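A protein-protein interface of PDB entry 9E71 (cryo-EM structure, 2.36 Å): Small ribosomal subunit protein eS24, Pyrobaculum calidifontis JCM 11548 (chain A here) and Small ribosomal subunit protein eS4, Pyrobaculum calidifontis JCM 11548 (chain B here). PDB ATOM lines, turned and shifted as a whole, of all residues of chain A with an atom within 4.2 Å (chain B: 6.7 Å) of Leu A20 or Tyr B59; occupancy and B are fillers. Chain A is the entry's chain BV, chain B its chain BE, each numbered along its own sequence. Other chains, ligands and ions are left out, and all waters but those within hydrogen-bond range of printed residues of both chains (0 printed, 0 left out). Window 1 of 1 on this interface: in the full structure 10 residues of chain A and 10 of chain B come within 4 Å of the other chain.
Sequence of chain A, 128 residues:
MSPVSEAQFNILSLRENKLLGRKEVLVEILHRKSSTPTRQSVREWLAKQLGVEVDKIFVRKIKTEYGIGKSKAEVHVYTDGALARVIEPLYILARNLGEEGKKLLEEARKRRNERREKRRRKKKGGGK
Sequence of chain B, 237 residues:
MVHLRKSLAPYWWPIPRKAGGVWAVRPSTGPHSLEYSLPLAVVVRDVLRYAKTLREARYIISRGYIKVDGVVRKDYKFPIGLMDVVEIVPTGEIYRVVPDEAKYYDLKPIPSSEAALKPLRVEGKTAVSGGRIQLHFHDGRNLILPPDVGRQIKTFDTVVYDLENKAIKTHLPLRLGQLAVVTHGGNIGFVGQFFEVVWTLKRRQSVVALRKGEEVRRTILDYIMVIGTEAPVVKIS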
ATOM      1  N   ASN A  17      15.758 -10.183  17.982  1.00  0.00           N
ATOM      2  CA  ASN A  17      14.365 -10.191  17.557  1.00  0.00           C
ATOM      3  C   ASN A  17      13.562  -9.521  18.664  1.00  0.00           C
ATOM      4  O   ASN A  17      13.263 -10.141  19.688  1.00  0.00           O
ATOM      5  CB  ASN A  17      13.889 -11.616  17.291  1.00  0.00           C
ATOM      6  CG  ASN A  17      12.583 -11.664  16.530  1.00  0.00           C
ATOM      7  OD1 ASN A  17      11.892 -10.657  16.393  1.00  0.00           O
ATOM      8  ND2 ASN A  17      12.238 -12.840  16.028  1.00  0.00           N
ATOM      9  N   LYS A  18      13.235  -8.243  18.468  1.00  0.00           N
ATOM     10  CA  LYS A  18      12.381  -7.547  19.421  1.00  0.00           C
ATOM     11  C   LYS A  18      10.935  -8.008  19.335  1.00  0.00           C
ATOM     12  O   LYS A  18      10.190  -7.847  20.306  1.00  0.00           O
ATOM     13  CB  LYS A  18      12.448  -6.039  19.191  1.00  0.00           C
ATOM     14  CG  LYS A  18      13.844  -5.470  19.228  1.00  0.00           C
ATOM     15  CD  LYS A  18      13.820  -3.962  19.088  1.00  0.00           C
ATOM     16  CE  LYS A  18      14.897  -3.486  18.133  1.00  0.00           C
ATOM     17  NZ  LYS A  18      14.846  -4.226  16.845  1.00  0.00           N
ATOM     18  N   LEU A  19      10.528  -8.565  18.192  1.00  0.00           N
ATOM     19  CA  LEU A  19       9.153  -9.022  18.028  1.00  0.00           C
ATOM     20  C   LEU A  19       8.831 -10.167  18.978  1.00  0.00           C
ATOM     21  O   LEU A  19       7.762 -10.184  19.598  1.00  0.00           O
ATOM     22  CB  LEU A  19       8.917  -9.448  16.581  1.00  0.00           C
ATOM     23  CG  LEU A  19       8.801  -8.316  15.562  1.00  0.00           C
ATOM     24  CD1 LEU A  19       8.775  -8.872  14.163  1.00  0.00           C
ATOM     25  CD2 LEU A  19       7.546  -7.530  15.823  1.00  0.00           C
ATOM     26  N   LEU A  20       9.738 -11.131  19.106  1.00  0.00           N
ATOM     27  CA  LEU A  20       9.564 -12.227  20.045  1.00  0.00           C
ATOM     28  C   LEU A  20      10.205 -11.938  21.392  1.00  0.00           C
ATOM     29  O   LEU A  20      10.143 -12.782  22.290  1.00  0.00           O
ATOM     30  CB  LEU A  20      10.129 -13.522  19.465  1.00  0.00           C
ATOM     31  CG  LEU A  20       9.505 -13.997  18.155  1.00  0.00           C
ATOM     32  CD1 LEU A  20      10.304 -15.144  17.560  1.00  0.00           C
ATOM     33  CD2 LEU A  20       8.063 -14.407  18.373  1.00  0.00           C
ATOM     34  N   GLY A  21      10.810 -10.766  21.552  1.00  0.00           N
ATOM     35  CA  GLY A  21      11.453 -10.419  22.807  1.00  0.00           C
ATOM     36  C   GLY A  21      12.624 -11.306  23.163  1.00  0.00           C
ATOM     37  O   GLY A  21      12.743 -11.739  24.315  1.00  0.00           O
ATOM     38  N   ARG A  22      13.496 -11.589  22.200  1.00  0.00           N
ATOM     39  CA  ARG A  22      14.624 -12.473  22.454  1.00  0.00           C
ATOM     40  C   ARG A  22      15.809 -12.055  21.597  1.00  0.00           C
ATOM     41  O   ARG A  22      15.708 -11.189  20.724  1.00  0.00           O
ATOM     42  CB  ARG A  22      14.264 -13.933  22.175  1.00  0.00           C
ATOM     43  CG  ARG A  22      14.236 -14.279  20.702  1.00  0.00           C
ATOM     44  CD  ARG A  22      13.326 -15.449  20.441  1.00  0.00           C
ATOM     45  NE  ARG A  22      13.373 -15.868  19.047  1.00  0.00           N
ATOM     46  CZ  ARG A  22      12.890 -17.018  18.600  1.00  0.00           C
ATOM     47  NH1 ARG A  22      12.334 -17.895  19.417  1.00  0.00           N
ATOM     48  NH2 ARG A  22      12.967 -17.292  17.302  1.00  0.00           N
ATOM     49  N   TYR A  78      16.141 -14.921  26.231  1.00  0.00           N
ATOM     50  CA  TYR A  78      14.853 -14.267  26.389  1.00  0.00           C
ATOM     51  C   TYR A  78      14.919 -13.197  27.467  1.00  0.00           C
ATOM     52  O   TYR A  78      15.661 -13.327  28.445  1.00  0.00           O
ATOM     53  CB  TYR A  78      13.773 -15.287  26.733  1.00  0.00           C
ATOM     54  CG  TYR A  78      13.292 -16.047  25.533  1.00  0.00           C
ATOM     55  CD1 TYR A  78      12.235 -15.576  24.769  1.00  0.00           C
ATOM     56  CD2 TYR A  78      13.900 -17.230  25.152  1.00  0.00           C
ATOM     57  CE1 TYR A  78      11.798 -16.263  23.669  1.00  0.00           C
ATOM     58  CE2 TYR A  78      13.467 -17.924  24.049  1.00  0.00           C
ATOM     59  CZ  TYR A  78      12.413 -17.437  23.312  1.00  0.00           C
ATOM     60  OH  TYR A  78      11.975 -18.125  22.209  1.00  0.00           O
ATOM     61  N   LEU A  83       7.496 -15.093  28.818  1.00  0.00           N
ATOM     62  CA  LEU A  83       7.447 -15.088  27.361  1.00  0.00           C
ATOM     63  C   LEU A  83       8.338 -16.176  26.782  1.00  0.00           C
ATOM     64  O   LEU A  83       8.030 -16.729  25.722  1.00  0.00           O
ATOM     65  CB  LEU A  83       7.843 -13.719  26.812  1.00  0.00           C
ATOM     66  CG  LEU A  83       7.803 -13.562  25.293  1.00  0.00           C
ATOM     67  CD1 LEU A  83       6.381 -13.663  24.784  1.00  0.00           C
ATOM     68  CD2 LEU A  83       8.431 -12.244  24.876  1.00  0.00           C
ATOM     69  N   ILE A  87       6.791 -18.910  24.294  1.00  0.00           N
ATOM     70  CA  ILE A  87       7.242 -18.882  22.908  1.00  0.00           C
ATOM     71  C   ILE A  87       7.949 -20.171  22.524  1.00  0.00           C
ATOM     72  O   ILE A  87       7.648 -20.764  21.485  1.00  0.00           O
ATOM     73  CB  ILE A  87       8.150 -17.659  22.672  1.00  0.00           C
ATOM     74  CG1 ILE A  87       7.354 -16.365  22.801  1.00  0.00           C
ATOM     75  CG2 ILE A  87       8.790 -17.739  21.305  1.00  0.00           C
ATOM     76  CD1 ILE A  87       8.050 -15.171  22.206  1.00  0.00           C
ATOM     77  N   TYR B  50      11.955 -12.956  10.945  1.00  0.00           N
ATOM     78  CA  TYR B  50      11.687 -12.693  12.353  1.00  0.00           C
ATOM     79  C   TYR B  50      11.188 -13.933  13.077  1.00  0.00           C
ATOM     80  O   TYR B  50      11.439 -14.088  14.276  1.00  0.00           O
ATOM     81  CB  TYR B  50      10.679 -11.557  12.493  1.00  0.00           C
ATOM     82  CG  TYR B  50      11.297 -10.189  12.387  1.00  0.00           C
ATOM     83  CD1 TYR B  50      12.240  -9.769  13.308  1.00  0.00           C
ATOM     84  CD2 TYR B  50      10.927  -9.312  11.379  1.00  0.00           C
ATOM     85  CE1 TYR B  50      12.807  -8.521  13.226  1.00  0.00           C
ATOM     86  CE2 TYR B  50      11.490  -8.060  11.287  1.00  0.00           C
ATOM     87  CZ  TYR B  50      12.431  -7.672  12.216  1.00  0.00           C
ATOM     88  OH  TYR B  50      13.002  -6.425  12.137  1.00  0.00           O
ATOM     89  N   ALA B  51      10.484 -14.816  12.379  1.00  0.00           N
ATOM     90  CA  ALA B  51       9.922 -16.016  12.977  1.00  0.00           C
ATOM     91  C   ALA B  51      10.503 -17.241  12.292  1.00  0.00           C
ATOM     92  O   ALA B  51      10.661 -17.263  11.070  1.00  0.00           O
ATOM     93  CB  ALA B  51       8.396 -16.029  12.871  1.00  0.00           C
ATOM     94  N   LYS B  52      10.818 -18.261  13.086  1.00  0.00           N
ATOM     95  CA  LYS B  52      11.429 -19.469  12.553  1.00  0.00           C
ATOM     96  C   LYS B  52      10.411 -20.510  12.116  1.00  0.00           C
ATOM     97  O   LYS B  52      10.742 -21.382  11.306  1.00  0.00           O
ATOM     98  CB  LYS B  52      12.373 -20.079  13.591  1.00  0.00           C
ATOM     99  CG  LYS B  52      13.576 -19.208  13.891  1.00  0.00           C
ATOM    100  CD  LYS B  52      14.637 -19.959  14.663  1.00  0.00           C
ATOM    101  CE  LYS B  52      15.913 -19.143  14.765  1.00  0.00           C
ATOM    102  NZ  LYS B  52      16.899 -19.762  15.689  1.00  0.00           N
ATOM    103  N   LEU B  54       5.876 -21.365  11.435  1.00  0.00           N
ATOM    104  CA  LEU B  54       4.547 -20.804  11.239  1.00  0.00           C
ATOM    105  C   LEU B  54       3.888 -20.458  12.564  1.00  0.00           C
ATOM    106  O   LEU B  54       3.140 -19.483  12.641  1.00  0.00           O
ATOM    107  CB  LEU B  54       3.669 -21.773  10.454  1.00  0.00           C
ATOM    108  CG  LEU B  54       2.351 -21.159   9.984  1.00  0.00           C
ATOM    109  CD1 LEU B  54       2.621 -20.097   8.941  1.00  0.00           C
ATOM    110  CD2 LEU B  54       1.407 -22.211   9.438  1.00  0.00           C
ATOM    111  N   ARG B  55       4.159 -21.235  13.615  1.00  0.00           N
ATOM    112  CA  ARG B  55       3.611 -20.930  14.933  1.00  0.00           C
ATOM    113  C   ARG B  55       4.130 -19.594  15.452  1.00  0.00           C
ATOM    114  O   ARG B  55       3.358 -18.763  15.941  1.00  0.00           O
ATOM    115  CB  ARG B  55       3.956 -22.052  15.912  1.00  0.00           C
ATOM    116  CG  ARG B  55       3.395 -23.406  15.534  1.00  0.00           C
ATOM    117  CD  ARG B  55       2.546 -23.993  16.651  1.00  0.00           C
ATOM    118  NE  ARG B  55       2.384 -25.436  16.518  1.00  0.00           N
ATOM    119  CZ  ARG B  55       2.122 -26.258  17.524  1.00  0.00           C
ATOM    120  NH1 ARG B  55       1.987 -25.815  18.762  1.00  0.00           N
ATOM    121  NH2 ARG B  55       1.985 -27.558  17.282  1.00  0.00           N
ATOM    122  N   GLU B  56       5.441 -19.366  15.344  1.00  0.00           N
ATOM    123  CA  GLU B  56       6.015 -18.109  15.812  1.00  0.00           C
ATOM    124  C   GLU B  56       5.548 -16.938  14.961  1.00  0.00           C
ATOM    125  O   GLU B  56       5.277 -15.850  15.486  1.00  0.00           O
ATOM    126  CB  GLU B  56       7.539 -18.198  15.817  1.00  0.00           C
ATOM    127  CG  GLU B  56       8.094 -19.126  16.878  1.00  0.00           C
ATOM    128  CD  GLU B  56       9.603 -19.262  16.807  1.00  0.00           C
ATOM    129  OE1 GLU B  56      10.228 -18.560  15.989  1.00  0.00           O
ATOM    130  OE2 GLU B  56      10.162 -20.081  17.563  1.00  0.00           O
ATOM    131  N   ALA B  57       5.448 -17.140  13.645  1.00  0.00           N
ATOM    132  CA  ALA B  57       4.936 -16.087  12.772  1.00  0.00           C
ATOM    133  C   ALA B  57       3.489 -15.744  13.106  1.00  0.00           C
ATOM    134  O   ALA B  57       3.110 -14.568  13.135  1.00  0.00           O
ATOM    135  CB  ALA B  57       5.063 -16.509  11.310  1.00  0.00           C
ATOM    136  N   ARG B  58       2.671 -16.759  13.379  1.00  0.00           N
ATOM    137  CA  ARG B  58       1.279 -16.513  13.725  1.00  0.00           C
ATOM    138  C   ARG B  58       1.162 -15.844  15.086  1.00  0.00           C
ATOM    139  O   ARG B  58       0.264 -15.025  15.296  1.00  0.00           O
ATOM    140  CB  ARG B  58       0.494 -17.819  13.690  1.00  0.00           C
ATOM    141  CG  ARG B  58      -0.075 -18.128  12.332  1.00  0.00           C
ATOM    142  CD  ARG B  58      -0.590 -19.538  12.259  1.00  0.00           C
ATOM    143  NE  ARG B  58      -2.029 -19.583  12.473  1.00  0.00           N
ATOM    144  CZ  ARG B  58      -2.689 -20.652  12.887  1.00  0.00           C
ATOM    145  NH1 ARG B  58      -2.071 -21.798  13.117  1.00  0.00           N
ATOM    146  NH2 ARG B  58      -4.001 -20.569  13.080  1.00  0.00           N
ATOM    147  N   TYR B  59       2.060 -16.172  16.018  1.00  0.00           N
ATOM    148  CA  TYR B  59       2.089 -15.465  17.296  1.00  0.00           C
ATOM    149  C   TYR B  59       2.396 -13.989  17.090  1.00  0.00           C
ATOM    150  O   TYR B  59       1.726 -13.114  17.658  1.00  0.00           O
ATOM    151  CB  TYR B  59       3.123 -16.106  18.228  1.00  0.00           C
ATOM    152  CG  TYR B  59       3.317 -15.372  19.540  1.00  0.00           C
ATOM    153  CD1 TYR B  59       4.341 -14.446  19.710  1.00  0.00           C
ATOM    154  CD2 TYR B  59       2.464 -15.599  20.605  1.00  0.00           C
ATOM    155  CE1 TYR B  59       4.497 -13.770  20.896  1.00  0.00           C
ATOM    156  CE2 TYR B  59       2.619 -14.935  21.795  1.00  0.00           C
ATOM    157  CZ  TYR B  59       3.634 -14.021  21.935  1.00  0.00           C
ATOM    158  OH  TYR B  59       3.784 -13.360  23.128  1.00  0.00           O
ATOM    159  N   ILE B  60       3.420 -13.699  16.282  1.00  0.00           N
ATOM    160  CA  ILE B  60       3.837 -12.320  16.045  1.00  0.00           C
ATOM    161  C   ILE B  60       2.723 -11.539  15.371  1.00  0.00           C
ATOM    162  O   ILE B  60       2.471 -10.374  15.697  1.00  0.00           O
ATOM    163  CB  ILE B  60       5.121 -12.285  15.203  1.00  0.00           C
ATOM    164  CG1 ILE B  60       6.306 -12.824  16.000  1.00  0.00           C
ATOM    165  CG2 ILE B  60       5.385 -10.875  14.722  1.00  0.00           C
ATOM    166  CD1 ILE B  60       7.516 -13.109  15.153  1.00  0.00           C
ATOM    167  N   ILE B  61       2.043 -12.169  14.414  1.00  0.00           N
ATOM    168  CA  ILE B  61       0.950 -11.499  13.725  1.00  0.00           C
ATOM    169  C   ILE B  61      -0.229 -11.288  14.663  1.00  0.00           C
ATOM    170  O   ILE B  61      -0.829 -10.209  14.690  1.00  0.00           O
ATOM    171  CB  ILE B  61       0.550 -12.296  12.472  1.00  0.00           C
ATOM    172  CG1 ILE B  61       1.558 -12.047  11.352  1.00  0.00           C
ATOM    173  CG2 ILE B  61      -0.840 -11.915  12.030  1.00  0.00           C
ATOM    174  CD1 ILE B  61       1.485 -13.048  10.235  1.00  0.00           C
ATOM    175  N   SER B  62      -0.572 -12.302  15.461  1.00  0.00           N
ATOM    176  CA  SER B  62      -1.718 -12.213  16.352  1.00  0.00           C
ATOM    177  C   SER B  62      -1.523 -11.188  17.455  1.00  0.00           C
ATOM    178  O   SER B  62      -2.512 -10.652  17.964  1.00  0.00           O
ATOM    179  CB  SER B  62      -2.009 -13.580  16.965  1.00  0.00           C
ATOM    180  OG  SER B  62      -2.626 -14.433  16.019  1.00  0.00           O
ATOM    181  N   ARG B  63      -0.279 -10.897  17.838  1.00  0.00           N
ATOM    182  CA  ARG B  63      -0.078  -9.816  18.798  1.00  0.00           C
ATOM    183  C   ARG B  63      -0.392  -8.437  18.228  1.00  0.00           C
ATOM    184  O   ARG B  63      -0.573  -7.497  19.007  1.00  0.00           O
ATOM    185  CB  ARG B  63       1.350  -9.827  19.334  1.00  0.00           C
ATOM    186  CG  ARG B  63       1.768 -11.148  19.915  1.00  0.00           C
ATOM    187  CD  ARG B  63       1.403 -11.233  21.379  1.00  0.00           C
ATOM    188  NE  ARG B  63      -0.028 -11.431  21.581  1.00  0.00           N
ATOM    189  CZ  ARG B  63      -0.691 -12.535  21.266  1.00  0.00           C
ATOM    190  NH1 ARG B  63      -0.088 -13.573  20.713  1.00  0.00           N
ATOM    191  NH2 ARG B  63      -1.996 -12.599  21.512  1.00  0.00           N
ATOM    192  N   GLY B  64      -0.475  -8.290  16.910  1.00  0.00           N
ATOM    193  CA  GLY B  64      -0.730  -6.989  16.329  1.00  0.00           C
ATOM    194  C   GLY B  64       0.506  -6.153  16.116  1.00  0.00           C
ATOM    195  O   GLY B  64       0.413  -4.926  16.046  1.00  0.00           O
ATOM    196  N   TYR B  65       1.672  -6.787  16.016  1.00  0.00           N
ATOM    197  CA  TYR B  65       2.917  -6.059  15.827  1.00  0.00           C
ATOM    198  C   TYR B  65       3.095  -5.557  14.404  1.00  0.00           C
ATOM    199  O   TYR B  65       3.914  -4.662  14.176  1.00  0.00           O
ATOM    200  CB  TYR B  65       4.099  -6.952  16.200  1.00  0.00           C
ATOM    201  CG  TYR B  65       4.223  -7.181  17.682  1.00  0.00           C
ATOM    202  CD1 TYR B  65       3.917  -6.176  18.584  1.00  0.00           C
ATOM    203  CD2 TYR B  65       4.628  -8.406  18.182  1.00  0.00           C
ATOM    204  CE1 TYR B  65       4.022  -6.380  19.934  1.00  0.00           C
ATOM    205  CE2 TYR B  65       4.733  -8.619  19.532  1.00  0.00           C
ATOM    206  CZ  TYR B  65       4.430  -7.602  20.404  1.00  0.00           C
ATOM    207  OH  TYR B  65       4.533  -7.806  21.757  1.00  0.00           O
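The backbone carbonyl oxygen (O) of Tyr B50 lies close to the side-chain amide nitrogen (ND2) of Asn A17 (2.3 Å).
OE1 of Glu B56 is in salt-bridge range of NH2 of Arg A22.
The backbone NH of Lys B52 lies within hydrogen-bond range of the side-chain carboxylate of Glu B56 (3.0 Å).
The guanidinium group (NH1) of Arg A22 sits at hydrogen-bond distance from the side-chain hydroxyl (OH) of Tyr A78 (2.8 Å).
The side-chain amide oxygen of Asn A17 lies within hydrogen-bond range of the backbone NH of Leu A20 (3.5 Å).
The backbone NH of Arg A22 is in hydrogen-bond range of the backbone carbonyl oxygen of Asn A17 (2.9 Å).
The side-chain amide oxygen of Asn A17 lies within hydrogen-bond range of the backbone NH of Leu A19 (3.1 Å).
Among the printed residues, pairs that only touch across the chains: Leu A83 with Tyr B59, Leu A20 with Ile B60, Leu A19 with Tyr B50, Leu A19 with Tyr B65, Leu A20 with Tyr B50, Leu A20 with Glu B56, Leu A20 with Tyr B59, Arg A22 with Lys B52 and Leu A19 with Ile B60.
Of the printed residues of chain B, Leu A20 touches Tyr B50, Glu B56, Tyr B59 and Ile B60.
Printed residues of chain A within 4 Å of Tyr B59: Leu A20 and Leu A83.
Printed residues of chain A within 4 Å of Tyr B65: Leu A19 (3.4 Å).
Printed residues of chain B within 4 Å of Arg A22: Lys B52 and Glu B56.
Gly B64 touches none of the printed residues of chain A.
Arg B63 touches none of the printed residues of chain A.
Printed residues of chain A that touch a printed residue of chain B: Asn A17, Leu A19, Leu A20, Arg A22 and Leu A83.
Of the 15 printed residues of chain B, 6 touch a printed residue of chain A.
Printed residues of chain B that touch a printed residue of chain A: Tyr B50, Lys B52, Glu B56, Tyr B59, Ile B60 and Tyr B65.
Along chain B the printed residues that touch a printed residue of chain A span positions 50 to 65.
Among the printed residues, 11 pairs touch across the chains.
Among the printed residues, Asp or Glu carboxylates within 4 Å of a Lys or Arg side-chain nitrogen of the other chain: Arg A22 with Glu B56.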
